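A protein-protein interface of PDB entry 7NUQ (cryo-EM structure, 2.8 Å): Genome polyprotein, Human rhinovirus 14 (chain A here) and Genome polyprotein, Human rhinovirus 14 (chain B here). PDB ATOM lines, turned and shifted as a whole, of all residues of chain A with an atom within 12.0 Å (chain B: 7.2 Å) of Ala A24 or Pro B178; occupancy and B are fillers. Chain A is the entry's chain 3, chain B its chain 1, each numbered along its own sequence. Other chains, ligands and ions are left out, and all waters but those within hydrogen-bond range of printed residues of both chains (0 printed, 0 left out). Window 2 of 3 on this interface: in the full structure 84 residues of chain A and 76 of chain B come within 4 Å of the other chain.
Among the printed residues, pairs that only touch across the chains: Pro A22 with Phe B190 (3.3 Å), Tyr A28 with Pro B193 (3.3 Å), Ser A21 with Arg B189 (3.4 Å), Pro A22 with Arg B189 (3.6 Å), Ala A24 with Ser B191 (3.7 Å), Leu A25 with Val B192 (3.7 Å), Ser A23 with Pro B193 (3.8 Å) and Ala A24 with Pro B178 (3.8 Å).
O of Pro A22 sits at hydrogen-bond distance from N of Ser B191, 3.2 Å away. O of Ser B191 sits at hydrogen-bond distance from OG of Ser A23 (2.6 Å).
N of Tyr B156 sits at hydrogen-bond distance from O of Pro B178.
Of the 10 printed residues of chain A, 6 touch a printed residue of chain B. Printed residues of chain A that touch a printed residue of chain B: Ser A21, Pro A22, Ser A23, Ala A24, Leu A25 and Tyr A28. Along chain A the printed residues that touch a printed residue of chain B span positions 21 to 28. Of the 19 printed residues of chain B, 6 touch a printed residue of chain A. Hydrophobic or aromatic side chains of chain B that line the printed part of chain A: Pro B178, Phe B190, Val B192 and Pro B193.
Of the printed residues of chain B, Ser A23 touches Ser B191 and Pro B193. Of chain B, only Pro B178 (3.8 Å) and Ser B191 (3.7 Å) come within 4 Å of Ala A24. Printed residues of chain B within 4 Å of Leu A25: Val B192 (3.7 Å). Asn A27 touches none of the printed residues of chain B. Of the printed residues of chain B, Tyr A28 touches Pro B193 (3.3 Å). No residue of chain A comes within 4 Å of Ala B154. No residue of chain A comes within 4 Å of Met B155. No residue of chain A comes within 4 Å of Tyr B156. Pro B158 touches none of the printed residues of chain A. No residue of chain A comes within 4 Å of Ser B174. No residue of chain A comes within 4 Å of Ser B176. Pro B178 touches one residue of chain A. No residue of chain A comes within 4 Å of Ser B179. Phe B190 touches one residue of chain A. Of the printed residues of chain A, Ser B191 touches Pro A22, Ser A23 and Ala A24. Printed residues of chain A within 4 Å of Val B192: Leu A25 (3.7 Å). The nearest residue of chain A that does not touch Pro B178 is Leu A25 (4.4 Å). The nearest printed residue of chain B that does not touch Tyr A28 is Val B192 (6.6 Å).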
ATOM      1  N   GLN A  20     -20.745  -1.458  38.037  1.00  0.00           N
ATOM      2  CA  GLN A  20     -20.568  -0.059  37.671  1.00  0.00           C
ATOM      3  C   GLN A  20     -19.134   0.194  37.219  1.00  0.00           C
ATOM      4  O   GLN A  20     -18.247  -0.646  37.398  1.00  0.00           O
ATOM      5  CB  GLN A  20     -20.904   0.847  38.856  1.00  0.00           C
ATOM      6  CG  GLN A  20     -22.208   0.513  39.571  1.00  0.00           C
ATOM      7  CD  GLN A  20     -22.437   1.381  40.797  1.00  0.00           C
ATOM      8  OE1 GLN A  20     -22.196   2.589  40.770  1.00  0.00           O
ATOM      9  NE2 GLN A  20     -22.900   0.766  41.880  1.00  0.00           N
ATOM     10  N   SER A  21     -18.904   1.365  36.629  1.00  0.00           N
ATOM     11  CA  SER A  21     -17.579   1.714  36.136  1.00  0.00           C
ATOM     12  C   SER A  21     -17.451   3.227  36.040  1.00  0.00           C
ATOM     13  O   SER A  21     -18.364   3.890  35.534  1.00  0.00           O
ATOM     14  CB  SER A  21     -17.313   1.085  34.762  1.00  0.00           C
ATOM     15  OG  SER A  21     -17.569  -0.308  34.781  1.00  0.00           O
ATOM     16  N   PRO A  22     -16.336   3.803  36.500  1.00  0.00           N
ATOM     17  CA  PRO A  22     -16.100   5.235  36.275  1.00  0.00           C
ATOM     18  C   PRO A  22     -15.749   5.511  34.820  1.00  0.00           C
ATOM     19  O   PRO A  22     -15.041   4.730  34.180  1.00  0.00           O
ATOM     20  CB  PRO A  22     -14.924   5.555  37.207  1.00  0.00           C
ATOM     21  CG  PRO A  22     -14.218   4.262  37.375  1.00  0.00           C
ATOM     22  CD  PRO A  22     -15.286   3.207  37.346  1.00  0.00           C
ATOM     23  N   SER A  23     -16.238   6.637  34.301  1.00  0.00           N
ATOM     24  CA  SER A  23     -16.081   6.948  32.887  1.00  0.00           C
ATOM     25  C   SER A  23     -14.964   7.964  32.675  1.00  0.00           C
ATOM     26  O   SER A  23     -14.801   8.897  33.465  1.00  0.00           O
ATOM     27  CB  SER A  23     -17.390   7.484  32.315  1.00  0.00           C
ATOM     28  OG  SER A  23     -17.350   7.504  30.900  1.00  0.00           O
ATOM     29  N   ALA A  24     -14.197   7.779  31.597  1.00  0.00           N
ATOM     30  CA  ALA A  24     -13.107   8.683  31.254  1.00  0.00           C
ATOM     31  C   ALA A  24     -13.551   9.851  30.384  1.00  0.00           C
ATOM     32  O   ALA A  24     -12.712  10.678  30.008  1.00  0.00           O
ATOM     33  CB  ALA A  24     -11.994   7.918  30.531  1.00  0.00           C
ATOM     34  N   LEU A  25     -14.839   9.940  30.054  1.00  0.00           N
ATOM     35  CA  LEU A  25     -15.387  11.024  29.244  1.00  0.00           C
ATOM     36  C   LEU A  25     -16.446  11.734  30.079  1.00  0.00           C
ATOM     37  O   LEU A  25     -17.650  11.476  29.929  1.00  0.00           O
ATOM     38  CB  LEU A  25     -15.955  10.495  27.929  1.00  0.00           C
ATOM     39  CG  LEU A  25     -14.881  10.016  26.950  1.00  0.00           C
ATOM     40  CD1 LEU A  25     -15.487   9.184  25.827  1.00  0.00           C
ATOM     41  CD2 LEU A  25     -14.122  11.202  26.384  1.00  0.00           C
ATOM     42  N   PRO A  26     -16.036  12.624  30.978  1.00  0.00           N
ATOM     43  CA  PRO A  26     -17.011  13.328  31.815  1.00  0.00           C
ATOM     44  C   PRO A  26     -17.775  14.387  31.040  1.00  0.00           C
ATOM     45  O   PRO A  26     -17.257  15.020  30.118  1.00  0.00           O
ATOM     46  CB  PRO A  26     -16.141  13.966  32.906  1.00  0.00           C
ATOM     47  CG  PRO A  26     -14.808  14.142  32.264  1.00  0.00           C
ATOM     48  CD  PRO A  26     -14.648  12.986  31.319  1.00  0.00           C
ATOM     49  N   ASN A  27     -19.035  14.563  31.428  1.00  0.00           N
ATOM     50  CA  ASN A  27     -19.954  15.564  30.900  1.00  0.00           C
ATOM     51  C   ASN A  27     -20.337  15.263  29.456  1.00  0.00           C
ATOM     52  O   ASN A  27     -21.016  16.091  28.830  1.00  0.00           O
ATOM     53  CB  ASN A  27     -19.379  16.986  30.980  1.00  0.00           C
ATOM     54  CG  ASN A  27     -19.315  17.503  32.403  1.00  0.00           C
ATOM     55  OD1 ASN A  27     -20.044  17.035  33.276  1.00  0.00           O
ATOM     56  ND2 ASN A  27     -18.441  18.474  32.642  1.00  0.00           N
ATOM     57  N   TYR A  28     -19.936  14.121  28.902  1.00  0.00           N
ATOM     58  CA  TYR A  28     -20.342  13.769  27.550  1.00  0.00           C
ATOM     59  C   TYR A  28     -21.838  13.485  27.521  1.00  0.00           C
ATOM     60  O   TYR A  28     -22.421  13.061  28.523  1.00  0.00           O
ATOM     61  CB  TYR A  28     -19.562  12.553  27.053  1.00  0.00           C
ATOM     62  CG  TYR A  28     -19.865  12.182  25.615  1.00  0.00           C
ATOM     63  CD1 TYR A  28     -19.112  12.698  24.570  1.00  0.00           C
ATOM     64  CD2 TYR A  28     -20.911  11.320  25.306  1.00  0.00           C
ATOM     65  CE1 TYR A  28     -19.387  12.362  23.256  1.00  0.00           C
ATOM     66  CE2 TYR A  28     -21.192  10.977  23.999  1.00  0.00           C
ATOM     67  CZ  TYR A  28     -20.429  11.501  22.976  1.00  0.00           C
ATOM     68  OH  TYR A  28     -20.712  11.161  21.673  1.00  0.00           O
ATOM     69  N   GLU A  29     -22.457  13.729  26.365  1.00  0.00           N
ATOM     70  CA  GLU A  29     -23.885  13.524  26.200  1.00  0.00           C
ATOM     71  C   GLU A  29     -24.131  12.588  25.028  1.00  0.00           C
ATOM     72  O   GLU A  29     -23.796  12.948  23.887  1.00  0.00           O
ATOM     73  CB  GLU A  29     -24.591  14.854  25.971  1.00  0.00           C
ATOM     74  CG  GLU A  29     -26.090  14.724  25.735  1.00  0.00           C
ATOM     75  CD  GLU A  29     -26.473  14.748  24.266  1.00  0.00           C
ATOM     76  OE1 GLU A  29     -25.576  14.868  23.407  1.00  0.00           O
ATOM     77  OE2 GLU A  29     -27.684  14.654  23.972  1.00  0.00           O
ATOM     78  N   GLN B 153       0.352   2.528  31.016  1.00  0.00           N
ATOM     79  CA  GLN B 153      -0.483   3.676  30.689  1.00  0.00           C
ATOM     80  C   GLN B 153      -1.302   3.344  29.445  1.00  0.00           C
ATOM     81  O   GLN B 153      -0.744   3.167  28.356  1.00  0.00           O
ATOM     82  CB  GLN B 153       0.371   4.924  30.465  1.00  0.00           C
ATOM     83  CG  GLN B 153      -0.422   6.192  30.166  1.00  0.00           C
ATOM     84  CD  GLN B 153       0.461   7.353  29.749  1.00  0.00           C
ATOM     85  OE1 GLN B 153       1.680   7.310  29.905  1.00  0.00           O
ATOM     86  NE2 GLN B 153      -0.154   8.398  29.211  1.00  0.00           N
ATOM     87  N   ALA B 154      -2.621   3.263  29.611  1.00  0.00           N
ATOM     88  CA  ALA B 154      -3.552   3.016  28.516  1.00  0.00           C
ATOM     89  C   ALA B 154      -4.180   4.352  28.136  1.00  0.00           C
ATOM     90  O   ALA B 154      -4.597   5.117  29.011  1.00  0.00           O
ATOM     91  CB  ALA B 154      -4.615   2.000  28.918  1.00  0.00           C
ATOM     92  N   MET B 155      -4.249   4.629  26.837  1.00  0.00           N
ATOM     93  CA  MET B 155      -4.592   5.951  26.334  1.00  0.00           C
ATOM     94  C   MET B 155      -5.645   5.838  25.238  1.00  0.00           C
ATOM     95  O   MET B 155      -5.515   5.011  24.329  1.00  0.00           O
ATOM     96  CB  MET B 155      -3.339   6.647  25.801  1.00  0.00           C
ATOM     97  CG  MET B 155      -3.484   8.131  25.526  1.00  0.00           C
ATOM     98  SD  MET B 155      -1.909   8.831  24.990  1.00  0.00           S
ATOM     99  CE  MET B 155      -2.332  10.555  24.764  1.00  0.00           C
ATOM    100  N   TYR B 156      -6.682   6.671  25.331  1.00  0.00           N
ATOM    101  CA  TYR B 156      -7.694   6.768  24.286  1.00  0.00           C
ATOM    102  C   TYR B 156      -7.297   7.876  23.319  1.00  0.00           C
ATOM    103  O   TYR B 156      -6.829   8.939  23.746  1.00  0.00           O
ATOM    104  CB  TYR B 156      -9.068   7.038  24.900  1.00  0.00           C
ATOM    105  CG  TYR B 156     -10.142   7.428  23.908  1.00  0.00           C
ATOM    106  CD1 TYR B 156     -10.439   8.763  23.664  1.00  0.00           C
ATOM    107  CD2 TYR B 156     -10.871   6.461  23.223  1.00  0.00           C
ATOM    108  CE1 TYR B 156     -11.421   9.127  22.763  1.00  0.00           C
ATOM    109  CE2 TYR B 156     -11.855   6.817  22.315  1.00  0.00           C
ATOM    110  CZ  TYR B 156     -12.126   8.151  22.092  1.00  0.00           C
ATOM    111  OH  TYR B 156     -13.103   8.516  21.195  1.00  0.00           O
ATOM    112  N   VAL B 157      -7.472   7.629  22.024  1.00  0.00           N
ATOM    113  CA  VAL B 157      -7.072   8.581  20.989  1.00  0.00           C
ATOM    114  C   VAL B 157      -8.292   8.946  20.150  1.00  0.00           C
ATOM    115  O   VAL B 157      -8.704   8.151  19.293  1.00  0.00           O
ATOM    116  CB  VAL B 157      -5.955   8.009  20.102  1.00  0.00           C
ATOM    117  CG1 VAL B 157      -5.301   9.121  19.288  1.00  0.00           C
ATOM    118  CG2 VAL B 157      -4.919   7.269  20.935  1.00  0.00           C
ATOM    119  N   PRO B 158      -8.905  10.111  20.354  1.00  0.00           N
ATOM    120  CA  PRO B 158     -10.042  10.508  19.508  1.00  0.00           C
ATOM    121  C   PRO B 158      -9.570  10.948  18.134  1.00  0.00           C
ATOM    122  O   PRO B 158      -8.391  11.287  17.955  1.00  0.00           O
ATOM    123  CB  PRO B 158     -10.674  11.672  20.284  1.00  0.00           C
ATOM    124  CG  PRO B 158      -9.549  12.244  21.085  1.00  0.00           C
ATOM    125  CD  PRO B 158      -8.669  11.073  21.447  1.00  0.00           C
ATOM    126  N   TRP B 172       1.689  11.633  25.595  1.00  0.00           N
ATOM    127  CA  TRP B 172       1.382  10.865  26.797  1.00  0.00           C
ATOM    128  C   TRP B 172       0.961  11.746  27.968  1.00  0.00           C
ATOM    129  O   TRP B 172       0.489  11.219  28.980  1.00  0.00           O
ATOM    130  CB  TRP B 172       2.585  10.005  27.195  1.00  0.00           C
ATOM    131  CG  TRP B 172       2.897   8.891  26.226  1.00  0.00           C
ATOM    132  CD1 TRP B 172       4.055   8.716  25.522  1.00  0.00           C
ATOM    133  CD2 TRP B 172       2.041   7.798  25.862  1.00  0.00           C
ATOM    134  NE1 TRP B 172       3.972   7.586  24.745  1.00  0.00           N
ATOM    135  CE2 TRP B 172       2.747   7.006  24.935  1.00  0.00           C
ATOM    136  CE3 TRP B 172       0.747   7.415  26.229  1.00  0.00           C
ATOM    137  CZ2 TRP B 172       2.202   5.852  24.370  1.00  0.00           C
ATOM    138  CZ3 TRP B 172       0.209   6.269  25.668  1.00  0.00           C
ATOM    139  CH2 TRP B 172       0.934   5.504  24.745  1.00  0.00           C
ATOM    140  N   SER B 174      -1.630  13.450  28.088  1.00  0.00           N
ATOM    141  CA  SER B 174      -3.011  12.983  28.202  1.00  0.00           C
ATOM    142  C   SER B 174      -3.922  14.060  28.788  1.00  0.00           C
ATOM    143  O   SER B 174      -4.882  13.771  29.506  1.00  0.00           O
ATOM    144  CB  SER B 174      -3.068  11.703  29.039  1.00  0.00           C
ATOM    145  OG  SER B 174      -2.205  10.714  28.503  1.00  0.00           O
ATOM    146  N   ALA B 175      -3.624  15.322  28.464  1.00  0.00           N
ATOM    147  CA  ALA B 175      -4.415  16.414  29.024  1.00  0.00           C
ATOM    148  C   ALA B 175      -5.852  16.373  28.519  1.00  0.00           C
ATOM    149  O   ALA B 175      -6.790  16.500  29.314  1.00  0.00           O
ATOM    150  CB  ALA B 175      -3.766  17.761  28.697  1.00  0.00           C
ATOM    151  N   SER B 176      -6.045  16.194  27.212  1.00  0.00           N
ATOM    152  CA  SER B 176      -7.355  15.883  26.656  1.00  0.00           C
ATOM    153  C   SER B 176      -7.526  14.414  26.316  1.00  0.00           C
ATOM    154  O   SER B 176      -8.653  13.911  26.395  1.00  0.00           O
ATOM    155  CB  SER B 176      -7.624  16.711  25.389  1.00  0.00           C
ATOM    156  OG  SER B 176      -8.101  18.006  25.703  1.00  0.00           O
ATOM    157  N   ASN B 177      -6.461  13.713  25.950  1.00  0.00           N
ATOM    158  CA  ASN B 177      -6.566  12.287  25.703  1.00  0.00           C
ATOM    159  C   ASN B 177      -6.764  11.548  27.025  1.00  0.00           C
ATOM    160  O   ASN B 177      -5.981  11.733  27.959  1.00  0.00           O
ATOM    161  CB  ASN B 177      -5.310  11.774  25.004  1.00  0.00           C
ATOM    162  CG  ASN B 177      -4.942  12.597  23.785  1.00  0.00           C
ATOM    163  OD1 ASN B 177      -3.782  12.956  23.593  1.00  0.00           O
ATOM    164  ND2 ASN B 177      -5.935  12.907  22.958  1.00  0.00           N
ATOM    165  N   PRO B 178      -7.804  10.722  27.145  1.00  0.00           N
ATOM    166  CA  PRO B 178      -7.968   9.933  28.372  1.00  0.00           C
ATOM    167  C   PRO B 178      -6.784   9.007  28.598  1.00  0.00           C
ATOM    168  O   PRO B 178      -6.290   8.362  27.669  1.00  0.00           O
ATOM    169  CB  PRO B 178      -9.256   9.138  28.119  1.00  0.00           C
ATOM    170  CG  PRO B 178      -9.979   9.890  27.057  1.00  0.00           C
ATOM    171  CD  PRO B 178      -8.926  10.528  26.210  1.00  0.00           C
ATOM    172  N   SER B 179      -6.330   8.945  29.847  1.00  0.00           N
ATOM    173  CA  SER B 179      -5.265   8.028  30.226  1.00  0.00           C
ATOM    174  C   SER B 179      -5.693   7.253  31.461  1.00  0.00           C
ATOM    175  O   SER B 179      -6.432   7.768  32.303  1.00  0.00           O
ATOM    176  CB  SER B 179      -3.950   8.761  30.504  1.00  0.00           C
ATOM    177  OG  SER B 179      -2.933   7.848  30.880  1.00  0.00           O
ATOM    178  N   VAL B 180      -5.227   6.011  31.552  1.00  0.00           N
ATOM    179  CA  VAL B 180      -5.465   5.153  32.705  1.00  0.00           C
ATOM    180  C   VAL B 180      -4.160   4.458  33.060  1.00  0.00           C
ATOM    181  O   VAL B 180      -3.598   3.718  32.246  1.00  0.00           O
ATOM    182  CB  VAL B 180      -6.572   4.115  32.436  1.00  0.00           C
ATOM    183  CG1 VAL B 180      -6.711   3.187  33.628  1.00  0.00           C
ATOM    184  CG2 VAL B 180      -7.894   4.808  32.129  1.00  0.00           C
ATOM    185  N   ARG B 189     -10.716  -0.210  34.008  1.00  0.00           N
ATOM    186  CA  ARG B 189     -12.157  -0.352  33.829  1.00  0.00           C
ATOM    187  C   ARG B 189     -12.748   1.040  33.663  1.00  0.00           C
ATOM    188  O   ARG B 189     -13.077   1.698  34.655  1.00  0.00           O
ATOM    189  CB  ARG B 189     -12.782  -1.087  35.012  1.00  0.00           C
ATOM    190  CG  ARG B 189     -14.282  -1.313  34.906  1.00  0.00           C
ATOM    191  CD  ARG B 189     -14.653  -2.179  33.718  1.00  0.00           C
ATOM    192  NE  ARG B 189     -14.137  -3.543  33.836  1.00  0.00           N
ATOM    193  CZ  ARG B 189     -14.802  -4.557  34.385  1.00  0.00           C
ATOM    194  NH1 ARG B 189     -16.020  -4.379  34.881  1.00  0.00           N
ATOM    195  NH2 ARG B 189     -14.241  -5.757  34.442  1.00  0.00           N
ATOM    196  N   PHE B 190     -12.887   1.482  32.412  1.00  0.00           N
ATOM    197  CA  PHE B 190     -13.465   2.782  32.108  1.00  0.00           C
ATOM    198  C   PHE B 190     -14.652   2.594  31.176  1.00  0.00           C
ATOM    199  O   PHE B 190     -14.611   1.766  30.262  1.00  0.00           O
ATOM    200  CB  PHE B 190     -12.438   3.735  31.473  1.00  0.00           C
ATOM    201  CG  PHE B 190     -11.782   3.200  30.230  1.00  0.00           C
ATOM    202  CD1 PHE B 190     -10.485   2.716  30.271  1.00  0.00           C
ATOM    203  CD2 PHE B 190     -12.454   3.193  29.016  1.00  0.00           C
ATOM    204  CE1 PHE B 190      -9.873   2.231  29.132  1.00  0.00           C
ATOM    205  CE2 PHE B 190     -11.846   2.702  27.871  1.00  0.00           C
ATOM    206  CZ  PHE B 190     -10.552   2.222  27.933  1.00  0.00           C
ATOM    207  N   SER B 191     -15.708   3.361  31.419  1.00  0.00           N
ATOM    208  CA  SER B 191     -16.903   3.297  30.596  1.00  0.00           C
ATOM    209  C   SER B 191     -16.858   4.369  29.518  1.00  0.00           C
ATOM    210  O   SER B 191     -16.245   5.426  29.689  1.00  0.00           O
ATOM    211  CB  SER B 191     -18.160   3.464  31.449  1.00  0.00           C
ATOM    212  OG  SER B 191     -19.323   3.210  30.680  1.00  0.00           O
ATOM    213  N   VAL B 192     -17.514   4.082  28.393  1.00  0.00           N
ATOM    214  CA  VAL B 192     -17.536   4.975  27.246  1.00  0.00           C
ATOM    215  C   VAL B 192     -18.984   5.134  26.798  1.00  0.00           C
ATOM    216  O   VAL B 192     -19.602   4.158  26.360  1.00  0.00           O
ATOM    217  CB  VAL B 192     -16.677   4.456  26.082  1.00  0.00           C
ATOM    218  CG1 VAL B 192     -16.238   5.605  25.193  1.00  0.00           C
ATOM    219  CG2 VAL B 192     -15.475   3.674  26.603  1.00  0.00           C
ATOM    220  N   PRO B 193     -19.575   6.322  26.886  1.00  0.00           N
ATOM    221  CA  PRO B 193     -20.909   6.518  26.311  1.00  0.00           C
ATOM    222  C   PRO B 193     -20.869   6.317  24.803  1.00  0.00           C
ATOM    223  O   PRO B 193     -19.812   6.344  24.173  1.00  0.00           O
ATOM    224  CB  PRO B 193     -21.262   7.958  26.695  1.00  0.00           C
ATOM    225  CG  PRO B 193     -19.951   8.618  26.952  1.00  0.00           C
ATOM    226  CD  PRO B 193     -19.045   7.562  27.485  1.00  0.00           C
